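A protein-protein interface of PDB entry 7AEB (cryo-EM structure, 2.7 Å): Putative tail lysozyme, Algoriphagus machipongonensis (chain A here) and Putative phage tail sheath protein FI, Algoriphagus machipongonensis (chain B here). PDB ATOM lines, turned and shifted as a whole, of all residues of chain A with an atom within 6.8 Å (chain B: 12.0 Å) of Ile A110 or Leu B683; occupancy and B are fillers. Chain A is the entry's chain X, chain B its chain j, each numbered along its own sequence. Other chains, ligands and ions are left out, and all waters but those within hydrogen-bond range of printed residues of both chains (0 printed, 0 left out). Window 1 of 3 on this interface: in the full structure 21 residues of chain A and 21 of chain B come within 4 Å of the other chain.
The backbone NH of Leu A108 is in hydrogen-bond range of the backbone carbonyl oxygen of Phe B680 (3.0 Å). The backbone NH (N) of Ile B682 sits at hydrogen-bond distance from the backbone carbonyl oxygen (O) of Leu A108. The backbone NH (N) of Ile A110 sits at hydrogen-bond distance from the backbone carbonyl oxygen (O) of Ile B682. N of Lys B684 is in hydrogen-bond range of O of Ile A110, at 3.2 Å. The side-chain hydroxyl of Ser B686 is in hydrogen-bond range of a ring nitrogen (NE2) of His A111 (3.4 Å). O of Lys B684 sits at hydrogen-bond distance from N of Leu A112, 3.0 Å away. The backbone NH (N) of Ser B686 is in hydrogen-bond range of the backbone carbonyl oxygen (O) of Leu A112.
O of Asp A97 is in hydrogen-bond range of N of His A111, 2.9 Å away. The backbone carbonyl oxygen (O) of Thr A99 is in hydrogen-bond range of the backbone NH (N) of Leu A109, 2.8 Å away.
Among the printed residues, merely in contact across the chains: Leu A112 with Phe B685, Ile A110 with Leu B683, Leu A108 with Ile B681, Leu A109 with Ile B682 and His A111 with Lys B684.
Of the printed residues of chain B, Ile A110 touches Ile B682, Leu B683 and Lys B684. Of chain A, only Ile A110 comes within 4 Å of Leu B683. No residue of chain B comes within 4 Å of Phe A43. No residue of chain B comes within 4 Å of Val A76. No residue of chain B comes within 4 Å of Ile A96. Asp A97 touches none of the printed residues of chain B. No residue of chain B comes within 4 Å of Thr A99. Leu A108 touches three residues of chain B. Of chain B, only Ile B682 comes within 4 Å of Leu A109. Of the printed residues of chain B, Leu A112 touches Lys B684 (3.0 Å), Phe B685 (3.4 Å) and Ser B686 (3.1 Å). Printed residues of chain A within 4 Å of Phe B685: Leu A112 (3.4 Å). Printed residues of chain A within 4 Å of Lys B684: Ile A110 (3.2 Å), His A111 (3.9 Å) and Leu A112 (3.0 Å). Leu A39 touches none of the printed residues of chain B. The nearest residue of chain A that does not touch Leu B683 is Phe A43 (4.1 Å).
Hydrophobic or aromatic side chains of chain A within 4 Å of the printed part of chain B: Leu A108, Leu A109, Ile A110, His A111 and Leu A112. Hydrophobic or aromatic side chains of chain B that line the printed part of chain A: Ile B682, Leu B683 and Phe B685. Among the printed residues, no Asp or Glu carboxylate lies within 4 Å of a Lys or Arg side-chain nitrogen of the other chain.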
ATOM      1  N   LEU A  39     -25.701  -6.956 -17.632  1.00  0.00           N
ATOM      2  CA  LEU A  39     -25.742  -8.386 -17.893  1.00  0.00           C
ATOM      3  C   LEU A  39     -26.793  -8.739 -18.934  1.00  0.00           C
ATOM      4  O   LEU A  39     -26.532  -9.563 -19.814  1.00  0.00           O
ATOM      5  CB  LEU A  39     -25.998  -9.146 -16.595  1.00  0.00           C
ATOM      6  CG  LEU A  39     -24.857  -9.185 -15.575  1.00  0.00           C
ATOM      7  CD1 LEU A  39     -25.362  -9.734 -14.258  1.00  0.00           C
ATOM      8  CD2 LEU A  39     -23.696 -10.033 -16.095  1.00  0.00           C
ATOM      9  N   PHE A  43     -25.594 -10.627 -22.698  1.00  0.00           N
ATOM     10  CA  PHE A  43     -26.031 -11.936 -23.142  1.00  0.00           C
ATOM     11  C   PHE A  43     -27.164 -11.876 -24.154  1.00  0.00           C
ATOM     12  O   PHE A  43     -27.701 -12.917 -24.528  1.00  0.00           O
ATOM     13  CB  PHE A  43     -26.396 -12.786 -21.929  1.00  0.00           C
ATOM     14  CG  PHE A  43     -25.186 -13.236 -21.156  1.00  0.00           C
ATOM     15  CD1 PHE A  43     -24.786 -12.592 -19.992  1.00  0.00           C
ATOM     16  CD2 PHE A  43     -24.416 -14.279 -21.631  1.00  0.00           C
ATOM     17  CE1 PHE A  43     -23.654 -13.004 -19.319  1.00  0.00           C
ATOM     18  CE2 PHE A  43     -23.291 -14.690 -20.964  1.00  0.00           C
ATOM     19  CZ  PHE A  43     -22.907 -14.054 -19.811  1.00  0.00           C
ATOM     20  N   SER A  44     -27.525 -10.689 -24.603  1.00  0.00           N
ATOM     21  CA  SER A  44     -28.463 -10.492 -25.694  1.00  0.00           C
ATOM     22  C   SER A  44     -27.832 -10.152 -27.015  1.00  0.00           C
ATOM     23  O   SER A  44     -28.565  -9.960 -27.989  1.00  0.00           O
ATOM     24  CB  SER A  44     -29.544  -9.461 -25.354  1.00  0.00           C
ATOM     25  OG  SER A  44     -30.157  -9.710 -24.117  1.00  0.00           O
ATOM     26  N   LEU A  60     -23.832 -18.355 -26.871  1.00  0.00           N
ATOM     27  CA  LEU A  60     -24.732 -19.379 -26.332  1.00  0.00           C
ATOM     28  C   LEU A  60     -25.601 -20.060 -27.403  1.00  0.00           C
ATOM     29  O   LEU A  60     -25.922 -21.241 -27.254  1.00  0.00           O
ATOM     30  CB  LEU A  60     -25.610 -18.779 -25.240  1.00  0.00           C
ATOM     31  CG  LEU A  60     -24.919 -18.430 -23.912  1.00  0.00           C
ATOM     32  CD1 LEU A  60     -25.879 -17.669 -23.033  1.00  0.00           C
ATOM     33  CD2 LEU A  60     -24.419 -19.680 -23.173  1.00  0.00           C
ATOM     34  N   VAL A  76     -21.077 -24.806 -21.428  1.00  0.00           N
ATOM     35  CA  VAL A  76     -21.922 -23.640 -21.115  1.00  0.00           C
ATOM     36  C   VAL A  76     -21.291 -22.791 -20.037  1.00  0.00           C
ATOM     37  O   VAL A  76     -21.250 -21.558 -20.135  1.00  0.00           O
ATOM     38  CB  VAL A  76     -23.319 -24.071 -20.635  1.00  0.00           C
ATOM     39  CG1 VAL A  76     -24.100 -22.873 -20.107  1.00  0.00           C
ATOM     40  CG2 VAL A  76     -24.083 -24.646 -21.676  1.00  0.00           C
ATOM     41  N   ILE A  80     -20.000 -18.696 -20.267  1.00  0.00           N
ATOM     42  CA  ILE A  80     -20.526 -17.645 -19.405  1.00  0.00           C
ATOM     43  C   ILE A  80     -19.410 -16.980 -18.626  1.00  0.00           C
ATOM     44  O   ILE A  80     -19.341 -15.749 -18.562  1.00  0.00           O
ATOM     45  CB  ILE A  80     -21.601 -18.206 -18.461  1.00  0.00           C
ATOM     46  CG1 ILE A  80     -22.824 -18.600 -19.281  1.00  0.00           C
ATOM     47  CG2 ILE A  80     -21.962 -17.185 -17.358  1.00  0.00           C
ATOM     48  CD1 ILE A  80     -23.841 -19.416 -18.542  1.00  0.00           C
ATOM     49  N   ILE A  96     -23.227 -21.269 -11.059  1.00  0.00           N
ATOM     50  CA  ILE A  96     -24.012 -21.466 -12.269  1.00  0.00           C
ATOM     51  C   ILE A  96     -24.722 -22.809 -12.168  1.00  0.00           C
ATOM     52  O   ILE A  96     -24.078 -23.859 -12.086  1.00  0.00           O
ATOM     53  CB  ILE A  96     -23.147 -21.373 -13.534  1.00  0.00           C
ATOM     54  CG1 ILE A  96     -22.491 -19.988 -13.593  1.00  0.00           C
ATOM     55  CG2 ILE A  96     -24.006 -21.612 -14.774  1.00  0.00           C
ATOM     56  CD1 ILE A  96     -21.422 -19.805 -14.651  1.00  0.00           C
ATOM     57  N   ASP A  97     -26.049 -22.772 -12.172  1.00  0.00           N
ATOM     58  CA  ASP A  97     -26.898 -23.945 -11.995  1.00  0.00           C
ATOM     59  C   ASP A  97     -27.650 -24.240 -13.315  1.00  0.00           C
ATOM     60  O   ASP A  97     -28.547 -23.485 -13.707  1.00  0.00           O
ATOM     61  CB  ASP A  97     -27.882 -23.670 -10.859  1.00  0.00           C
ATOM     62  CG  ASP A  97     -28.605 -24.894 -10.404  1.00  0.00           C
ATOM     63  OD1 ASP A  97     -28.785 -25.819 -11.193  1.00  0.00           O
ATOM     64  OD2 ASP A  97     -29.244 -24.845  -9.346  1.00  0.00           O
ATOM     65  N   ILE A  98     -27.337 -25.364 -13.969  1.00  0.00           N
ATOM     66  CA  ILE A  98     -27.920 -25.709 -15.275  1.00  0.00           C
ATOM     67  C   ILE A  98     -28.819 -26.937 -15.164  1.00  0.00           C
ATOM     68  O   ILE A  98     -28.335 -28.035 -14.869  1.00  0.00           O
ATOM     69  CB  ILE A  98     -26.838 -25.962 -16.328  1.00  0.00           C
ATOM     70  CG1 ILE A  98     -25.948 -24.739 -16.455  1.00  0.00           C
ATOM     71  CG2 ILE A  98     -27.494 -26.304 -17.658  1.00  0.00           C
ATOM     72  CD1 ILE A  98     -24.719 -24.959 -17.255  1.00  0.00           C
ATOM     73  N   THR A  99     -30.124 -26.763 -15.429  1.00  0.00           N
ATOM     74  CA  THR A  99     -31.102 -27.858 -15.313  1.00  0.00           C
ATOM     75  C   THR A  99     -32.169 -27.884 -16.419  1.00  0.00           C
ATOM     76  O   THR A  99     -32.411 -26.896 -17.109  1.00  0.00           O
ATOM     77  CB  THR A  99     -31.812 -27.828 -13.948  1.00  0.00           C
ATOM     78  OG1 THR A  99     -32.744 -28.913 -13.872  1.00  0.00           O
ATOM     79  CG2 THR A  99     -32.543 -26.516 -13.741  1.00  0.00           C
ATOM     80  N   LEU A 108     -33.984 -25.448 -21.690  1.00  0.00           N
ATOM     81  CA  LEU A 108     -32.814 -25.550 -20.836  1.00  0.00           C
ATOM     82  C   LEU A 108     -32.860 -24.345 -19.911  1.00  0.00           C
ATOM     83  O   LEU A 108     -33.054 -23.221 -20.374  1.00  0.00           O
ATOM     84  CB  LEU A 108     -31.523 -25.568 -21.666  1.00  0.00           C
ATOM     85  CG  LEU A 108     -30.174 -25.696 -20.942  1.00  0.00           C
ATOM     86  CD1 LEU A 108     -30.060 -27.048 -20.290  1.00  0.00           C
ATOM     87  CD2 LEU A 108     -29.013 -25.502 -21.907  1.00  0.00           C
ATOM     88  N   LEU A 109     -32.714 -24.567 -18.612  1.00  0.00           N
ATOM     89  CA  LEU A 109     -32.845 -23.494 -17.634  1.00  0.00           C
ATOM     90  C   LEU A 109     -31.505 -23.194 -16.979  1.00  0.00           C
ATOM     91  O   LEU A 109     -30.920 -24.063 -16.331  1.00  0.00           O
ATOM     92  CB  LEU A 109     -33.858 -23.888 -16.570  1.00  0.00           C
ATOM     93  CG  LEU A 109     -35.233 -24.300 -17.078  1.00  0.00           C
ATOM     94  CD1 LEU A 109     -36.060 -24.783 -15.907  1.00  0.00           C
ATOM     95  CD2 LEU A 109     -35.922 -23.154 -17.794  1.00  0.00           C
ATOM     96  N   ILE A 110     -31.029 -21.960 -17.100  1.00  0.00           N
ATOM     97  CA  ILE A 110     -29.735 -21.599 -16.531  1.00  0.00           C
ATOM     98  C   ILE A 110     -29.903 -20.494 -15.502  1.00  0.00           C
ATOM     99  O   ILE A 110     -30.371 -19.399 -15.830  1.00  0.00           O
ATOM    100  CB  ILE A 110     -28.736 -21.172 -17.614  1.00  0.00           C
ATOM    101  CG1 ILE A 110     -28.572 -22.301 -18.632  1.00  0.00           C
ATOM    102  CG2 ILE A 110     -27.402 -20.816 -16.961  1.00  0.00           C
ATOM    103  CD1 ILE A 110     -27.794 -21.948 -19.858  1.00  0.00           C
ATOM    104  N   HIS A 111     -29.458 -20.745 -14.276  1.00  0.00           N
ATOM    105  CA  HIS A 111     -29.548 -19.759 -13.198  1.00  0.00           C
ATOM    106  C   HIS A 111     -28.153 -19.291 -12.767  1.00  0.00           C
ATOM    107  O   HIS A 111     -27.370 -20.071 -12.216  1.00  0.00           O
ATOM    108  CB  HIS A 111     -30.336 -20.352 -12.034  1.00  0.00           C
ATOM    109  CG  HIS A 111     -30.574 -19.415 -10.889  1.00  0.00           C
ATOM    110  ND1 HIS A 111     -31.022 -19.868  -9.669  1.00  0.00           N
ATOM    111  CD2 HIS A 111     -30.454 -18.072 -10.770  1.00  0.00           C
ATOM    112  CE1 HIS A 111     -31.158 -18.848  -8.845  1.00  0.00           C
ATOM    113  NE2 HIS A 111     -30.817 -17.747  -9.486  1.00  0.00           N
ATOM    114  N   LEU A 112     -27.855 -18.010 -12.998  1.00  0.00           N
ATOM    115  CA  LEU A 112     -26.575 -17.407 -12.623  1.00  0.00           C
ATOM    116  C   LEU A 112     -26.707 -16.587 -11.350  1.00  0.00           C
ATOM    117  O   LEU A 112     -27.498 -15.643 -11.291  1.00  0.00           O
ATOM    118  CB  LEU A 112     -26.020 -16.487 -13.717  1.00  0.00           C
ATOM    119  CG  LEU A 112     -24.770 -15.625 -13.356  1.00  0.00           C
ATOM    120  CD1 LEU A 112     -23.539 -16.475 -13.106  1.00  0.00           C
ATOM    121  CD2 LEU A 112     -24.468 -14.592 -14.439  1.00  0.00           C
ATOM    122  N   ALA B 678     -33.163 -29.685 -27.336  1.00  0.00           N
ATOM    123  CA  ALA B 678     -33.501 -28.423 -26.691  1.00  0.00           C
ATOM    124  C   ALA B 678     -33.733 -27.344 -27.741  1.00  0.00           C
ATOM    125  O   ALA B 678     -32.910 -27.173 -28.636  1.00  0.00           O
ATOM    126  CB  ALA B 678     -32.392 -27.983 -25.756  1.00  0.00           C
ATOM    127  N   GLU B 679     -34.818 -26.586 -27.604  1.00  0.00           N
ATOM    128  CA  GLU B 679     -35.102 -25.490 -28.525  1.00  0.00           C
ATOM    129  C   GLU B 679     -34.993 -24.113 -27.887  1.00  0.00           C
ATOM    130  O   GLU B 679     -34.784 -23.130 -28.597  1.00  0.00           O
ATOM    131  CB  GLU B 679     -36.499 -25.636 -29.144  1.00  0.00           C
ATOM    132  CG  GLU B 679     -36.674 -26.810 -30.093  1.00  0.00           C
ATOM    133  CD  GLU B 679     -38.090 -26.918 -30.660  1.00  0.00           C
ATOM    134  OE1 GLU B 679     -38.995 -27.213 -29.899  1.00  0.00           O
ATOM    135  OE2 GLU B 679     -38.287 -26.745 -31.853  1.00  0.00           O
ATOM    136  N   PHE B 680     -35.145 -24.015 -26.578  1.00  0.00           N
ATOM    137  CA  PHE B 680     -35.182 -22.717 -25.937  1.00  0.00           C
ATOM    138  C   PHE B 680     -34.206 -22.659 -24.783  1.00  0.00           C
ATOM    139  O   PHE B 680     -34.006 -23.649 -24.088  1.00  0.00           O
ATOM    140  CB  PHE B 680     -36.581 -22.433 -25.419  1.00  0.00           C
ATOM    141  CG  PHE B 680     -37.619 -22.533 -26.475  1.00  0.00           C
ATOM    142  CD1 PHE B 680     -38.390 -23.665 -26.577  1.00  0.00           C
ATOM    143  CD2 PHE B 680     -37.799 -21.535 -27.394  1.00  0.00           C
ATOM    144  CE1 PHE B 680     -39.325 -23.790 -27.561  1.00  0.00           C
ATOM    145  CE2 PHE B 680     -38.736 -21.665 -28.381  1.00  0.00           C
ATOM    146  CZ  PHE B 680     -39.496 -22.794 -28.463  1.00  0.00           C
ATOM    147  N   ILE B 681     -33.636 -21.482 -24.555  1.00  0.00           N
ATOM    148  CA  ILE B 681     -32.744 -21.243 -23.431  1.00  0.00           C
ATOM    149  C   ILE B 681     -33.258 -20.090 -22.608  1.00  0.00           C
ATOM    150  O   ILE B 681     -33.442 -18.989 -23.121  1.00  0.00           O
ATOM    151  CB  ILE B 681     -31.316 -20.948 -23.897  1.00  0.00           C
ATOM    152  CG1 ILE B 681     -30.778 -22.159 -24.671  1.00  0.00           C
ATOM    153  CG2 ILE B 681     -30.424 -20.569 -22.697  1.00  0.00           C
ATOM    154  CD1 ILE B 681     -29.475 -21.938 -25.372  1.00  0.00           C
ATOM    155  N   ILE B 682     -33.456 -20.322 -21.323  1.00  0.00           N
ATOM    156  CA  ILE B 682     -33.967 -19.291 -20.445  1.00  0.00           C
ATOM    157  C   ILE B 682     -32.940 -18.943 -19.381  1.00  0.00           C
ATOM    158  O   ILE B 682     -32.488 -19.817 -18.644  1.00  0.00           O
ATOM    159  CB  ILE B 682     -35.280 -19.746 -19.812  1.00  0.00           C
ATOM    160  CG1 ILE B 682     -36.289 -20.027 -20.938  1.00  0.00           C
ATOM    161  CG2 ILE B 682     -35.787 -18.683 -18.843  1.00  0.00           C
ATOM    162  CD1 ILE B 682     -37.537 -20.715 -20.509  1.00  0.00           C
ATOM    163  N   LEU B 683     -32.588 -17.668 -19.290  1.00  0.00           N
ATOM    164  CA  LEU B 683     -31.624 -17.208 -18.305  1.00  0.00           C
ATOM    165  C   LEU B 683     -32.281 -16.431 -17.186  1.00  0.00           C
ATOM    166  O   LEU B 683     -33.298 -15.776 -17.385  1.00  0.00           O
ATOM    167  CB  LEU B 683     -30.584 -16.302 -18.935  1.00  0.00           C
ATOM    168  CG  LEU B 683     -29.784 -16.866 -20.088  1.00  0.00           C
ATOM    169  CD1 LEU B 683     -28.880 -15.787 -20.596  1.00  0.00           C
ATOM    170  CD2 LEU B 683     -28.982 -18.065 -19.642  1.00  0.00           C
ATOM    171  N   LYS B 684     -31.653 -16.492 -16.015  1.00  0.00           N
ATOM    172  CA  LYS B 684     -32.078 -15.748 -14.840  1.00  0.00           C
ATOM    173  C   LYS B 684     -30.837 -15.270 -14.088  1.00  0.00           C
ATOM    174  O   LYS B 684     -29.839 -15.986 -14.018  1.00  0.00           O
ATOM    175  CB  LYS B 684     -32.949 -16.620 -13.935  1.00  0.00           C
ATOM    176  CG  LYS B 684     -33.432 -15.921 -12.675  1.00  0.00           C
ATOM    177  CD  LYS B 684     -34.281 -16.841 -11.821  1.00  0.00           C
ATOM    178  CE  LYS B 684     -34.750 -16.143 -10.555  1.00  0.00           C
ATOM    179  NZ  LYS B 684     -35.570 -14.936 -10.855  1.00  0.00           N
ATOM    180  N   PHE B 685     -30.891 -14.067 -13.527  1.00  0.00           N
ATOM    181  CA  PHE B 685     -29.781 -13.527 -12.755  1.00  0.00           C
ATOM    182  C   PHE B 685     -30.222 -13.104 -11.366  1.00  0.00           C
ATOM    183  O   PHE B 685     -31.320 -12.608 -11.213  1.00  0.00           O
ATOM    184  CB  PHE B 685     -29.201 -12.278 -13.411  1.00  0.00           C
ATOM    185  CG  PHE B 685     -28.784 -12.451 -14.828  1.00  0.00           C
ATOM    186  CD1 PHE B 685     -29.419 -11.753 -15.835  1.00  0.00           C
ATOM    187  CD2 PHE B 685     -27.733 -13.271 -15.156  1.00  0.00           C
ATOM    188  CE1 PHE B 685     -29.033 -11.896 -17.145  1.00  0.00           C
ATOM    189  CE2 PHE B 685     -27.346 -13.418 -16.469  1.00  0.00           C
ATOM    190  CZ  PHE B 685     -27.998 -12.735 -17.461  1.00  0.00           C
ATOM    191  N   SER B 686     -29.368 -13.288 -10.354  1.00  0.00           N
ATOM    192  CA  SER B 686     -29.648 -12.799  -9.015  1.00  0.00           C
ATOM    193  C   SER B 686     -28.315 -12.428  -8.373  1.00  0.00           C
ATOM    194  O   SER B 686     -27.267 -12.959  -8.739  1.00  0.00           O
ATOM    195  CB  SER B 686     -30.329 -13.846  -8.155  1.00  0.00           C
ATOM    196  OG  SER B 686     -29.529 -14.977  -7.992  1.00  0.00           O
ATOM    197  N   HIS B 687     -28.368 -11.566  -7.372  1.00  0.00           N
ATOM    198  CA  HIS B 687     -27.170 -11.054  -6.745  1.00  0.00           C
ATOM    199  C   HIS B 687     -27.221 -10.995  -5.230  1.00  0.00           C
ATOM    200  O   HIS B 687     -28.273 -11.043  -4.623  1.00  0.00           O
ATOM    201  CB  HIS B 687     -26.958  -9.640  -7.223  1.00  0.00           C
ATOM    202  CG  HIS B 687     -27.671  -8.627  -6.392  1.00  0.00           C
ATOM    203  ND1 HIS B 687     -28.996  -8.304  -6.587  1.00  0.00           N
ATOM    204  CD2 HIS B 687     -27.246  -7.861  -5.359  1.00  0.00           C
ATOM    205  CE1 HIS B 687     -29.359  -7.400  -5.701  1.00  0.00           C
ATOM    206  NE2 HIS B 687     -28.315  -7.113  -4.946  1.00  0.00           N
